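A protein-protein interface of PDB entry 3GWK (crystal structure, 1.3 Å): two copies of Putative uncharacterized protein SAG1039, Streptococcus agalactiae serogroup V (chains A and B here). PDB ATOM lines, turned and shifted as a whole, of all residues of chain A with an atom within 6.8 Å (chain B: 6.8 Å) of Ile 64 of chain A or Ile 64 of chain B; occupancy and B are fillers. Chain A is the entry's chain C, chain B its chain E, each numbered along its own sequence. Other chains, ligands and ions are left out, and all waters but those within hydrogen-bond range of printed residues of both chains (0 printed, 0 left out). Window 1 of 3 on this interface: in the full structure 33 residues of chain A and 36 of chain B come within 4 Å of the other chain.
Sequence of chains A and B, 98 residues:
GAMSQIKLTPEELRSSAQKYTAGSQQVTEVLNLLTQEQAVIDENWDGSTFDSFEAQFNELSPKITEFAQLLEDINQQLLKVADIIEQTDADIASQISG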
ATOM      1  N   VAL A  27     -11.745  23.211 -21.753  1.00  0.00           N
ATOM      2  CA  VAL A  27     -10.329  22.836 -21.833  1.00  0.00           C
ATOM      3  C   VAL A  27      -9.935  22.023 -20.576  1.00  0.00           C
ATOM      4  O   VAL A  27      -9.263  20.983 -20.683  1.00  0.00           O
ATOM      5  CB  VAL A  27      -9.448  24.125 -21.994  1.00  0.00           C
ATOM      6  CG1 VAL A  27      -7.948  23.819 -21.842  1.00  0.00           C
ATOM      7  CG2 VAL A  27      -9.693  24.768 -23.362  1.00  0.00           C
ATOM      8  N   THR A  28     -10.322  22.496 -19.409  1.00  0.00           N
ATOM      9  CA  THR A  28     -10.016  21.786 -18.174  1.00  0.00           C
ATOM     10  C   THR A  28     -10.576  20.401 -18.203  1.00  0.00           C
ATOM     11  O   THR A  28      -9.907  19.434 -17.781  1.00  0.00           O
ATOM     12  CB  THR A  28     -10.541  22.599 -16.954  1.00  0.00           C
ATOM     13  OG1 THR A  28      -9.792  23.812 -16.908  1.00  0.00           O
ATOM     14  CG2 THR A  28     -10.393  21.808 -15.644  1.00  0.00           C
ATOM     15  N   VAL A  30     -11.333  18.475 -20.825  1.00  0.00           N
ATOM     16  CA  VAL A  30     -10.586  17.648 -21.773  1.00  0.00           C
ATOM     17  C   VAL A  30      -9.274  17.206 -21.110  1.00  0.00           C
ATOM     18  O   VAL A  30      -8.898  16.016 -21.145  1.00  0.00           O
ATOM     19  CB  VAL A  30     -10.311  18.364 -23.090  1.00  0.00           C
ATOM     20  CG1 VAL A  30      -9.298  17.508 -23.943  1.00  0.00           C
ATOM     21  CG2 VAL A  30     -11.569  18.587 -23.859  1.00  0.00           C
ATOM     22  N   LEU A  31      -8.571  18.153 -20.522  1.00  0.00           N
ATOM     23  CA  LEU A  31      -7.266  17.801 -19.939  1.00  0.00           C
ATOM     24  C   LEU A  31      -7.430  16.780 -18.807  1.00  0.00           C
ATOM     25  O   LEU A  31      -6.679  15.812 -18.718  1.00  0.00           O
ATOM     26  CB  LEU A  31      -6.576  19.060 -19.448  1.00  0.00           C
ATOM     27  CG  LEU A  31      -5.150  18.802 -18.894  1.00  0.00           C
ATOM     28  CD1 LEU A  31      -4.199  18.288 -19.975  1.00  0.00           C
ATOM     29  CD2 LEU A  31      -4.646  20.101 -18.279  1.00  0.00           C
ATOM     30  N   PHE A  57       2.941  14.838 -23.914  1.00  0.00           N
ATOM     31  CA  PHE A  57       1.725  15.167 -23.209  1.00  0.00           C
ATOM     32  C   PHE A  57       2.131  15.894 -21.911  1.00  0.00           C
ATOM     33  O   PHE A  57       1.570  16.907 -21.529  1.00  0.00           O
ATOM     34  CB  PHE A  57       0.934  13.902 -22.948  1.00  0.00           C
ATOM     35  CG  PHE A  57      -0.426  14.152 -22.354  1.00  0.00           C
ATOM     36  CD1 PHE A  57      -0.570  14.479 -21.013  1.00  0.00           C
ATOM     37  CD2 PHE A  57      -1.559  14.121 -23.150  1.00  0.00           C
ATOM     38  CE1 PHE A  57      -1.851  14.693 -20.517  1.00  0.00           C
ATOM     39  CE2 PHE A  57      -2.819  14.381 -22.650  1.00  0.00           C
ATOM     40  CZ  PHE A  57      -2.979  14.646 -21.338  1.00  0.00           C
ATOM     41  N   GLU A  59       4.818  17.481 -21.123  1.00  0.00           N
ATOM     42  CA  GLU A  59       5.404  18.810 -21.392  1.00  0.00           C
ATOM     43  C   GLU A  59       4.321  19.858 -21.760  1.00  0.00           C
ATOM     44  O   GLU A  59       4.412  21.099 -21.423  1.00  0.00           O
ATOM     45  CB  GLU A  59       6.348  18.702 -22.566  1.00  0.00           C
ATOM     46  CG  GLU A  59       7.128  19.945 -22.869  1.00  0.00           C
ATOM     47  CD  GLU A  59       8.271  19.697 -23.858  1.00  0.00           C
ATOM     48  OE1 GLU A  59       8.128  20.087 -25.038  1.00  0.00           O
ATOM     49  OE2 GLU A  59       9.264  19.091 -23.442  1.00  0.00           O
ATOM     50  N   LEU A  60       3.294  19.441 -22.487  1.00  0.00           N
ATOM     51  CA  LEU A  60       2.263  20.402 -22.939  1.00  0.00           C
ATOM     52  C   LEU A  60       1.201  20.639 -21.890  1.00  0.00           C
ATOM     53  O   LEU A  60       0.590  21.735 -21.878  1.00  0.00           O
ATOM     54  CB  LEU A  60       1.613  19.835 -24.209  1.00  0.00           C
ATOM     55  CG  LEU A  60       2.510  20.048 -25.440  1.00  0.00           C
ATOM     56  CD1 LEU A  60       1.939  19.228 -26.586  1.00  0.00           C
ATOM     57  CD2 LEU A  60       2.578  21.513 -25.798  1.00  0.00           C
ATOM     58  N   SER A  61       0.929  19.635 -21.074  1.00  0.00           N
ATOM     59  CA  SER A  61      -0.123  19.627 -20.022  1.00  0.00           C
ATOM     60  C   SER A  61      -0.141  20.977 -19.203  1.00  0.00           C
ATOM     61  O   SER A  61      -1.198  21.657 -19.183  1.00  0.00           O
ATOM     62  CB  SER A  61      -0.140  18.376 -19.121  1.00  0.00           C
ATOM     63  OG  SER A  61      -1.183  18.457 -18.077  1.00  0.00           O
ATOM     64  N   PRO A  62       1.002  21.425 -18.673  1.00  0.00           N
ATOM     65  CA  PRO A  62       0.937  22.691 -17.901  1.00  0.00           C
ATOM     66  C   PRO A  62       0.569  23.906 -18.744  1.00  0.00           C
ATOM     67  O   PRO A  62      -0.052  24.813 -18.213  1.00  0.00           O
ATOM     68  CB  PRO A  62       2.384  22.868 -17.348  1.00  0.00           C
ATOM     69  CG  PRO A  62       3.066  21.620 -17.633  1.00  0.00           C
ATOM     70  CD  PRO A  62       2.348  20.811 -18.630  1.00  0.00           C
ATOM     71  N   LYS A  63       0.855  23.906 -20.051  1.00  0.00           N
ATOM     72  CA  LYS A  63       0.433  24.956 -20.949  1.00  0.00           C
ATOM     73  C   LYS A  63      -1.066  24.969 -21.160  1.00  0.00           C
ATOM     74  O   LYS A  63      -1.677  26.010 -21.209  1.00  0.00           O
ATOM     75  CB  LYS A  63       1.153  24.787 -22.286  1.00  0.00           C
ATOM     76  CG  LYS A  63       2.687  24.823 -22.068  1.00  0.00           C
ATOM     77  CD  LYS A  63       3.193  26.310 -22.238  1.00  0.00           C
ATOM     78  CE  LYS A  63       3.488  27.116 -21.079  1.00  0.00           C
ATOM     79  NZ  LYS A  63       4.958  27.418 -21.157  1.00  0.00           N
ATOM     80  N   ILE A  64      -1.654  23.805 -21.193  1.00  0.00           N
ATOM     81  CA  ILE A  64      -3.098  23.688 -21.275  1.00  0.00           C
ATOM     82  C   ILE A  64      -3.763  24.208 -19.976  1.00  0.00           C
ATOM     83  O   ILE A  64      -4.753  24.969 -20.031  1.00  0.00           O
ATOM     84  CB  ILE A  64      -3.498  22.221 -21.553  1.00  0.00           C
ATOM     85  CG1 ILE A  64      -2.716  21.703 -22.783  1.00  0.00           C
ATOM     86  CG2 ILE A  64      -5.037  22.183 -21.766  1.00  0.00           C
ATOM     87  CD1 ILE A  64      -2.709  22.599 -24.035  1.00  0.00           C
ATOM     88  N   THR A  65      -3.174  23.844 -18.829  1.00  0.00           N
ATOM     89  CA  THR A  65      -3.663  24.389 -17.557  1.00  0.00           C
ATOM     90  C   THR A  65      -3.554  25.918 -17.540  1.00  0.00           C
ATOM     91  O   THR A  65      -4.512  26.617 -17.152  1.00  0.00           O
ATOM     92  CB  THR A  65      -2.919  23.755 -16.409  1.00  0.00           C
ATOM     93  OG1 THR A  65      -3.141  22.344 -16.416  1.00  0.00           O
ATOM     94  CG2 THR A  65      -3.376  24.343 -15.036  1.00  0.00           C
ATOM     95  N   GLU A  66      -2.439  26.435 -18.011  1.00  0.00           N
ATOM     96  CA  GLU A  66      -2.277  27.898 -18.057  1.00  0.00           C
ATOM     97  C   GLU A  66      -3.303  28.526 -18.972  1.00  0.00           C
ATOM     98  O   GLU A  66      -3.801  29.626 -18.714  1.00  0.00           O
ATOM     99  CB  GLU A  66      -0.896  28.375 -18.512  1.00  0.00           C
ATOM    100  CG  GLU A  66      -0.732  30.000 -18.592  1.00  0.00           C
ATOM    101  CD  GLU A  66      -1.149  30.704 -17.316  1.00  0.00           C
ATOM    102  OE1 GLU A  66      -1.739  31.701 -17.304  1.00  0.00           O
ATOM    103  OE2 GLU A  66      -0.986  30.142 -16.233  1.00  0.00           O
ATOM    104  N   PHE A  67      -3.562  27.880 -20.099  1.00  0.00           N
ATOM    105  CA  PHE A  67      -4.523  28.442 -21.025  1.00  0.00           C
ATOM    106  C   PHE A  67      -5.892  28.498 -20.378  1.00  0.00           C
ATOM    107  O   PHE A  67      -6.592  29.508 -20.485  1.00  0.00           O
ATOM    108  CB  PHE A  67      -4.528  27.578 -22.290  1.00  0.00           C
ATOM    109  CG  PHE A  67      -5.369  28.137 -23.445  1.00  0.00           C
ATOM    110  CD1 PHE A  67      -5.054  29.369 -24.060  1.00  0.00           C
ATOM    111  CD2 PHE A  67      -6.457  27.432 -23.951  1.00  0.00           C
ATOM    112  CE1 PHE A  67      -5.775  29.813 -25.133  1.00  0.00           C
ATOM    113  CE2 PHE A  67      -7.173  27.923 -25.031  1.00  0.00           C
ATOM    114  CZ  PHE A  67      -6.834  29.134 -25.597  1.00  0.00           C
ATOM    115  N   ALA A  68      -6.319  27.431 -19.768  1.00  0.00           N
ATOM    116  CA  ALA A  68      -7.615  27.451 -19.042  1.00  0.00           C
ATOM    117  C   ALA A  68      -7.628  28.568 -18.016  1.00  0.00           C
ATOM    118  O   ALA A  68      -8.614  29.263 -17.845  1.00  0.00           O
ATOM    119  CB  ALA A  68      -7.911  26.099 -18.422  1.00  0.00           C
ATOM    120  N   GLN A  69      -6.553  28.727 -17.276  1.00  0.00           N
ATOM    121  CA  GLN A  69      -6.490  29.784 -16.264  1.00  0.00           C
ATOM    122  C   GLN A  69      -6.559  31.169 -16.916  1.00  0.00           C
ATOM    123  O   GLN A  69      -7.264  32.078 -16.441  1.00  0.00           O
ATOM    124  CB  GLN A  69      -5.219  29.579 -15.412  1.00  0.00           C
ATOM    125  CG  GLN A  69      -5.432  30.247 -13.924  1.00  0.00           C
ATOM    126  CD  GLN A  69      -6.661  29.530 -12.941  1.00  0.00           C
ATOM    127  OE1 GLN A  69      -7.950  29.869 -13.057  1.00  0.00           O
ATOM    128  NE2 GLN A  69      -6.245  28.670 -11.949  1.00  0.00           N
ATOM    129  N   VAL B  27     -10.762  21.058 -28.056  1.00  0.00           N
ATOM    130  CA  VAL B  27      -9.690  22.048 -27.819  1.00  0.00           C
ATOM    131  C   VAL B  27      -9.547  22.987 -29.029  1.00  0.00           C
ATOM    132  O   VAL B  27      -9.458  24.226 -28.897  1.00  0.00           O
ATOM    133  CB  VAL B  27      -8.352  21.333 -27.524  1.00  0.00           C
ATOM    134  CG1 VAL B  27      -7.229  22.295 -27.578  1.00  0.00           C
ATOM    135  CG2 VAL B  27      -8.463  20.662 -26.149  1.00  0.00           C
ATOM    136  N   THR B  28      -9.588  22.439 -30.226  1.00  0.00           N
ATOM    137  CA  THR B  28      -9.476  23.264 -31.432  1.00  0.00           C
ATOM    138  C   THR B  28     -10.683  24.226 -31.562  1.00  0.00           C
ATOM    139  O   THR B  28     -10.491  25.389 -31.861  1.00  0.00           O
ATOM    140  CB  THR B  28      -9.379  22.372 -32.645  1.00  0.00           C
ATOM    141  OG1 THR B  28      -8.091  21.760 -32.594  1.00  0.00           O
ATOM    142  CG2 THR B  28      -9.497  23.177 -33.938  1.00  0.00           C
ATOM    143  N   VAL B  30     -12.437  25.548 -29.098  1.00  0.00           N
ATOM    144  CA  VAL B  30     -12.263  26.621 -28.110  1.00  0.00           C
ATOM    145  C   VAL B  30     -11.210  27.580 -28.650  1.00  0.00           C
ATOM    146  O   VAL B  30     -11.406  28.826 -28.623  1.00  0.00           O
ATOM    147  CB  VAL B  30     -11.825  26.058 -26.743  1.00  0.00           C
ATOM    148  CG1 VAL B  30     -11.475  27.255 -25.778  1.00  0.00           C
ATOM    149  CG2 VAL B  30     -12.993  25.244 -26.100  1.00  0.00           C
ATOM    150  N   LEU B  31     -10.055  27.072 -29.117  1.00  0.00           N
ATOM    151  CA  LEU B  31      -9.035  27.972 -29.646  1.00  0.00           C
ATOM    152  C   LEU B  31      -9.561  28.782 -30.787  1.00  0.00           C
ATOM    153  O   LEU B  31      -9.332  30.011 -30.894  1.00  0.00           O
ATOM    154  CB  LEU B  31      -7.801  27.170 -30.027  1.00  0.00           C
ATOM    155  CG  LEU B  31      -6.628  28.032 -30.509  1.00  0.00           C
ATOM    156  CD1 LEU B  31      -6.066  28.911 -29.399  1.00  0.00           C
ATOM    157  CD2 LEU B  31      -5.509  27.139 -31.034  1.00  0.00           C
ATOM    158  N   PHE B  57      -2.263  35.219 -24.474  1.00  0.00           N
ATOM    159  CA  PHE B  57      -3.029  34.373 -25.369  1.00  0.00           C
ATOM    160  C   PHE B  57      -2.152  33.936 -26.560  1.00  0.00           C
ATOM    161  O   PHE B  57      -2.122  32.746 -26.923  1.00  0.00           O
ATOM    162  CB  PHE B  57      -4.276  35.079 -25.842  1.00  0.00           C
ATOM    163  CG  PHE B  57      -5.248  34.177 -26.562  1.00  0.00           C
ATOM    164  CD1 PHE B  57      -5.041  33.843 -27.893  1.00  0.00           C
ATOM    165  CD2 PHE B  57      -6.384  33.701 -25.897  1.00  0.00           C
ATOM    166  CE1 PHE B  57      -6.016  33.069 -28.551  1.00  0.00           C
ATOM    167  CE2 PHE B  57      -7.314  32.902 -26.602  1.00  0.00           C
ATOM    168  CZ  PHE B  57      -7.126  32.608 -27.884  1.00  0.00           C
ATOM    169  N   GLU B  59       1.060  33.716 -26.841  1.00  0.00           N
ATOM    170  CA  GLU B  59       2.155  32.851 -26.478  1.00  0.00           C
ATOM    171  C   GLU B  59       1.693  31.452 -26.316  1.00  0.00           C
ATOM    172  O   GLU B  59       2.371  30.500 -26.725  1.00  0.00           O
ATOM    173  CB  GLU B  59       2.744  33.325 -25.155  1.00  0.00           C
ATOM    174  CG  GLU B  59       4.117  32.785 -24.887  1.00  0.00           C
ATOM    175  CD  GLU B  59       5.265  33.731 -25.334  1.00  0.00           C
ATOM    176  OE1 GLU B  59       6.360  33.643 -24.733  1.00  0.00           O
ATOM    177  OE2 GLU B  59       5.082  34.549 -26.281  1.00  0.00           O
ATOM    178  N   LEU B  60       0.519  31.272 -25.738  1.00  0.00           N
ATOM    179  CA  LEU B  60       0.040  29.942 -25.521  1.00  0.00           C
ATOM    180  C   LEU B  60      -0.555  29.257 -26.774  1.00  0.00           C
ATOM    181  O   LEU B  60      -0.502  28.027 -26.912  1.00  0.00           O
ATOM    182  CB  LEU B  60      -1.007  29.943 -24.412  1.00  0.00           C
ATOM    183  CG  LEU B  60      -0.362  30.206 -23.051  1.00  0.00           C
ATOM    184  CD1 LEU B  60      -1.460  30.508 -22.026  1.00  0.00           C
ATOM    185  CD2 LEU B  60       0.388  28.986 -22.603  1.00  0.00           C
ATOM    186  N   SER B  61      -1.164  30.059 -27.647  1.00  0.00           N
ATOM    187  CA  SER B  61      -1.912  29.552 -28.777  1.00  0.00           C
ATOM    188  C   SER B  61      -1.181  28.403 -29.525  1.00  0.00           C
ATOM    189  O   SER B  61      -1.781  27.360 -29.765  1.00  0.00           O
ATOM    190  CB  SER B  61      -2.234  30.692 -29.708  1.00  0.00           C
ATOM    191  OG  SER B  61      -2.860  30.197 -30.885  1.00  0.00           O
ATOM    192  N   PRO B  62       0.097  28.580 -29.926  1.00  0.00           N
ATOM    193  CA  PRO B  62       0.730  27.507 -30.693  1.00  0.00           C
ATOM    194  C   PRO B  62       0.853  26.221 -29.904  1.00  0.00           C
ATOM    195  O   PRO B  62       0.845  25.138 -30.498  1.00  0.00           O
ATOM    196  CB  PRO B  62       2.165  28.085 -31.022  1.00  0.00           C
ATOM    197  CG  PRO B  62       2.177  29.397 -30.482  1.00  0.00           C
ATOM    198  CD  PRO B  62       0.926  29.799 -29.854  1.00  0.00           C
ATOM    199  N   LYS B  63       0.999  26.294 -28.576  1.00  0.00           N
ATOM    200  CA  LYS B  63       1.024  25.128 -27.743  1.00  0.00           C
ATOM    201  C   LYS B  63      -0.325  24.437 -27.717  1.00  0.00           C
ATOM    202  O   LYS B  63      -0.384  23.224 -27.638  1.00  0.00           O
ATOM    203  CB  LYS B  63       1.420  25.479 -26.283  1.00  0.00           C
ATOM    204  CG  LYS B  63       2.727  26.197 -26.174  1.00  0.00           C
ATOM    205  CD  LYS B  63       3.854  25.353 -26.683  1.00  0.00           C
ATOM    206  CE  LYS B  63       5.213  26.074 -26.301  1.00  0.00           C
ATOM    207  NZ  LYS B  63       6.308  25.466 -27.086  1.00  0.00           N
ATOM    208  N   ILE B  64      -1.374  25.229 -27.776  1.00  0.00           N
ATOM    209  CA  ILE B  64      -2.673  24.624 -27.800  1.00  0.00           C
ATOM    210  C   ILE B  64      -2.887  23.836 -29.126  1.00  0.00           C
ATOM    211  O   ILE B  64      -3.410  22.733 -29.142  1.00  0.00           O
ATOM    212  CB  ILE B  64      -3.783  25.726 -27.649  1.00  0.00           C
ATOM    213  CG1 ILE B  64      -3.457  26.675 -26.525  1.00  0.00           C
ATOM    214  CG2 ILE B  64      -5.115  24.990 -27.422  1.00  0.00           C
ATOM    215  CD1 ILE B  64      -3.257  25.976 -25.206  1.00  0.00           C
ATOM    216  N   THR B  65      -2.516  24.458 -30.223  1.00  0.00           N
ATOM    217  CA  THR B  65      -2.508  23.784 -31.526  1.00  0.00           C
ATOM    218  C   THR B  65      -1.649  22.519 -31.502  1.00  0.00           C
ATOM    219  O   THR B  65      -2.103  21.438 -31.926  1.00  0.00           O
ATOM    220  CB  THR B  65      -1.979  24.714 -32.591  1.00  0.00           C
ATOM    221  OG1 THR B  65      -2.856  25.835 -32.725  1.00  0.00           O
ATOM    222  CG2 THR B  65      -1.812  24.065 -33.950  1.00  0.00           C
ATOM    223  N   GLU B  66      -0.482  22.572 -30.857  1.00  0.00           N
ATOM    224  CA  GLU B  66       0.370  21.364 -30.767  1.00  0.00           C
ATOM    225  C   GLU B  66      -0.307  20.286 -29.931  1.00  0.00           C
ATOM    226  O   GLU B  66      -0.212  19.073 -30.273  1.00  0.00           O
ATOM    227  CB  GLU B  66       1.648  21.742 -30.116  1.00  0.00           C
ATOM    228  CG  GLU B  66       2.622  22.467 -31.010  1.00  0.00           C
ATOM    229  CD  GLU B  66       3.839  23.019 -30.215  1.00  0.00           C
ATOM    230  OE1 GLU B  66       4.327  22.310 -29.291  1.00  0.00           O
ATOM    231  OE2 GLU B  66       4.267  24.150 -30.532  1.00  0.00           O
ATOM    232  N   PHE B  67      -0.953  20.686 -28.836  1.00  0.00           N
ATOM    233  CA  PHE B  67      -1.653  19.746 -28.016  1.00  0.00           C
ATOM    234  C   PHE B  67      -2.750  19.047 -28.796  1.00  0.00           C
ATOM    235  O   PHE B  67      -2.895  17.836 -28.744  1.00  0.00           O
ATOM    236  CB  PHE B  67      -2.166  20.415 -26.764  1.00  0.00           C
ATOM    237  CG  PHE B  67      -2.799  19.513 -25.752  1.00  0.00           C
ATOM    238  CD1 PHE B  67      -4.158  19.548 -25.483  1.00  0.00           C
ATOM    239  CD2 PHE B  67      -2.026  18.619 -24.996  1.00  0.00           C
ATOM    240  CE1 PHE B  67      -4.707  18.763 -24.505  1.00  0.00           C
ATOM    241  CE2 PHE B  67      -2.602  17.830 -24.036  1.00  0.00           C
ATOM    242  CZ  PHE B  67      -3.947  17.920 -23.778  1.00  0.00           C
ATOM    243  N   ALA B  68      -3.570  19.822 -29.493  1.00  0.00           N
ATOM    244  CA  ALA B  68      -4.651  19.215 -30.239  1.00  0.00           C
ATOM    245  C   ALA B  68      -4.061  18.236 -31.280  1.00  0.00           C
ATOM    246  O   ALA B  68      -4.681  17.169 -31.528  1.00  0.00           O
ATOM    247  CB  ALA B  68      -5.443  20.294 -30.940  1.00  0.00           C
ATOM    248  N   GLN B  69      -2.932  18.556 -31.912  1.00  0.00           N
ATOM    249  CA  GLN B  69      -2.359  17.650 -32.851  1.00  0.00           C
ATOM    250  C   GLN B  69      -1.836  16.377 -32.185  1.00  0.00           C
ATOM    251  O   GLN B  69      -1.987  15.274 -32.731  1.00  0.00           O
ATOM    252  CB  GLN B  69      -1.244  18.332 -33.625  1.00  0.00           C
ATOM    253  CG  GLN B  69      -0.618  17.458 -34.708  1.00  0.00           C
ATOM    254  CD  GLN B  69      -1.595  17.087 -35.798  1.00  0.00           C
ATOM    255  OE1 GLN B  69      -1.823  15.876 -36.075  1.00  0.00           O
ATOM    256  NE2 GLN B  69      -2.159  18.031 -36.420  1.00  0.00           N
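Among the printed residues, pairs that only touch across the chains: Val 27 of chain A with Val 30 of chain B (3.9 Å), Val 30 of chain A with Val 27 of chain B (3.9 Å), Leu 31 of chain A with Phe 67 of chain B (3.8 Å), Phe 57 of chain A with Phe 67 of chain B (3.7 Å), Leu 60 of chain A with Lys 63 of chain B (3.9 Å), Leu 60 of chain A with Glu 66 of chain B (3.99 Å), Leu 60 of chain A with Phe 67 of chain B (3.9 Å), Lys 63 of chain A with Leu 60 of chain B (3.9 Å), Lys 63 of chain A with Lys 63 of chain B (3.97 Å), Ile 64 of chain A with Ile 64 of chain B (3.6 Å), Ile 64 of chain A with Phe 67 of chain B (3.5 Å), Glu 66 of chain A with Leu 60 of chain B (3.5 Å), Phe 67 of chain A with Leu 31 of chain B (3.9 Å), Phe 67 of chain A with Phe 57 of chain B (3.8 Å), Phe 67 of chain A with Leu 60 of chain B (3.8 Å) and Phe 67 of chain A with Ile 64 of chain B (3.5 Å).
Printed residues of chain B within 4 Å of Leu 31 of chain A: Phe 67.
Of the printed residues of chain B, Leu 60 of chain A touches Lys 63, Glu 66 and Phe 67.
Ile 64 of chain A touches just these residues of chain B: Ile 64 (3.6 Å) and Phe 67 (3.5 Å).
Ile 64 of chain B touches just these residues of chain A: Ile 64 (3.6 Å) and Phe 67 (3.5 Å).
The nearest residue of chain B that does not touch Ile 64 of chain A is Lys 63 of chain B (4.3 Å).
The nearest printed residue of chain B that does not touch Leu 31 of chain A is Val 27 of chain B (6.2 Å).
Hydrophobic or aromatic side chains of chain B within 4 Å of the printed part of chain A: Val 27, Val 30, Leu 31, Phe 57, Leu 60, Ile 64 and Phe 67.
Printed residues of chain A that touch a printed residue of chain B: Val 27, Val 30, Leu 31, Phe 57, Leu 60, Lys 63, Ile 64, Glu 66 and Phe 67.
Hydrophobic or aromatic side chains of chain A that line the printed part of chain B: Val 27, Val 30, Leu 31, Phe 57, Leu 60, Ile 64 and Phe 67.
Val 27 of chain A touches Val 30 of chain B, and with the chains exchanged Val 30 of chain A touches Val 27 of chain B.
Leu 60 of chain A touches Glu 66 of chain B, and with the chains exchanged Glu 66 of chain A touches Leu 60 of chain B.
Leu 60 of chain A touches Phe 67 of chain B, and with the chains exchanged Phe 67 of chain A touches Leu 60 of chain B.
Lys 63 of chain B touches its own counterpart, Lys 63 of chain A.
Positions printed for both chains: 27, 28, 30, 31, 57, 59, 60, 61, 62, 63, 64, 65, 66, 67, 68 and 69.
Of the 16 pairs that touch across the chains among the printed residues, 16 have their exchanged pair printed and touching as well.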
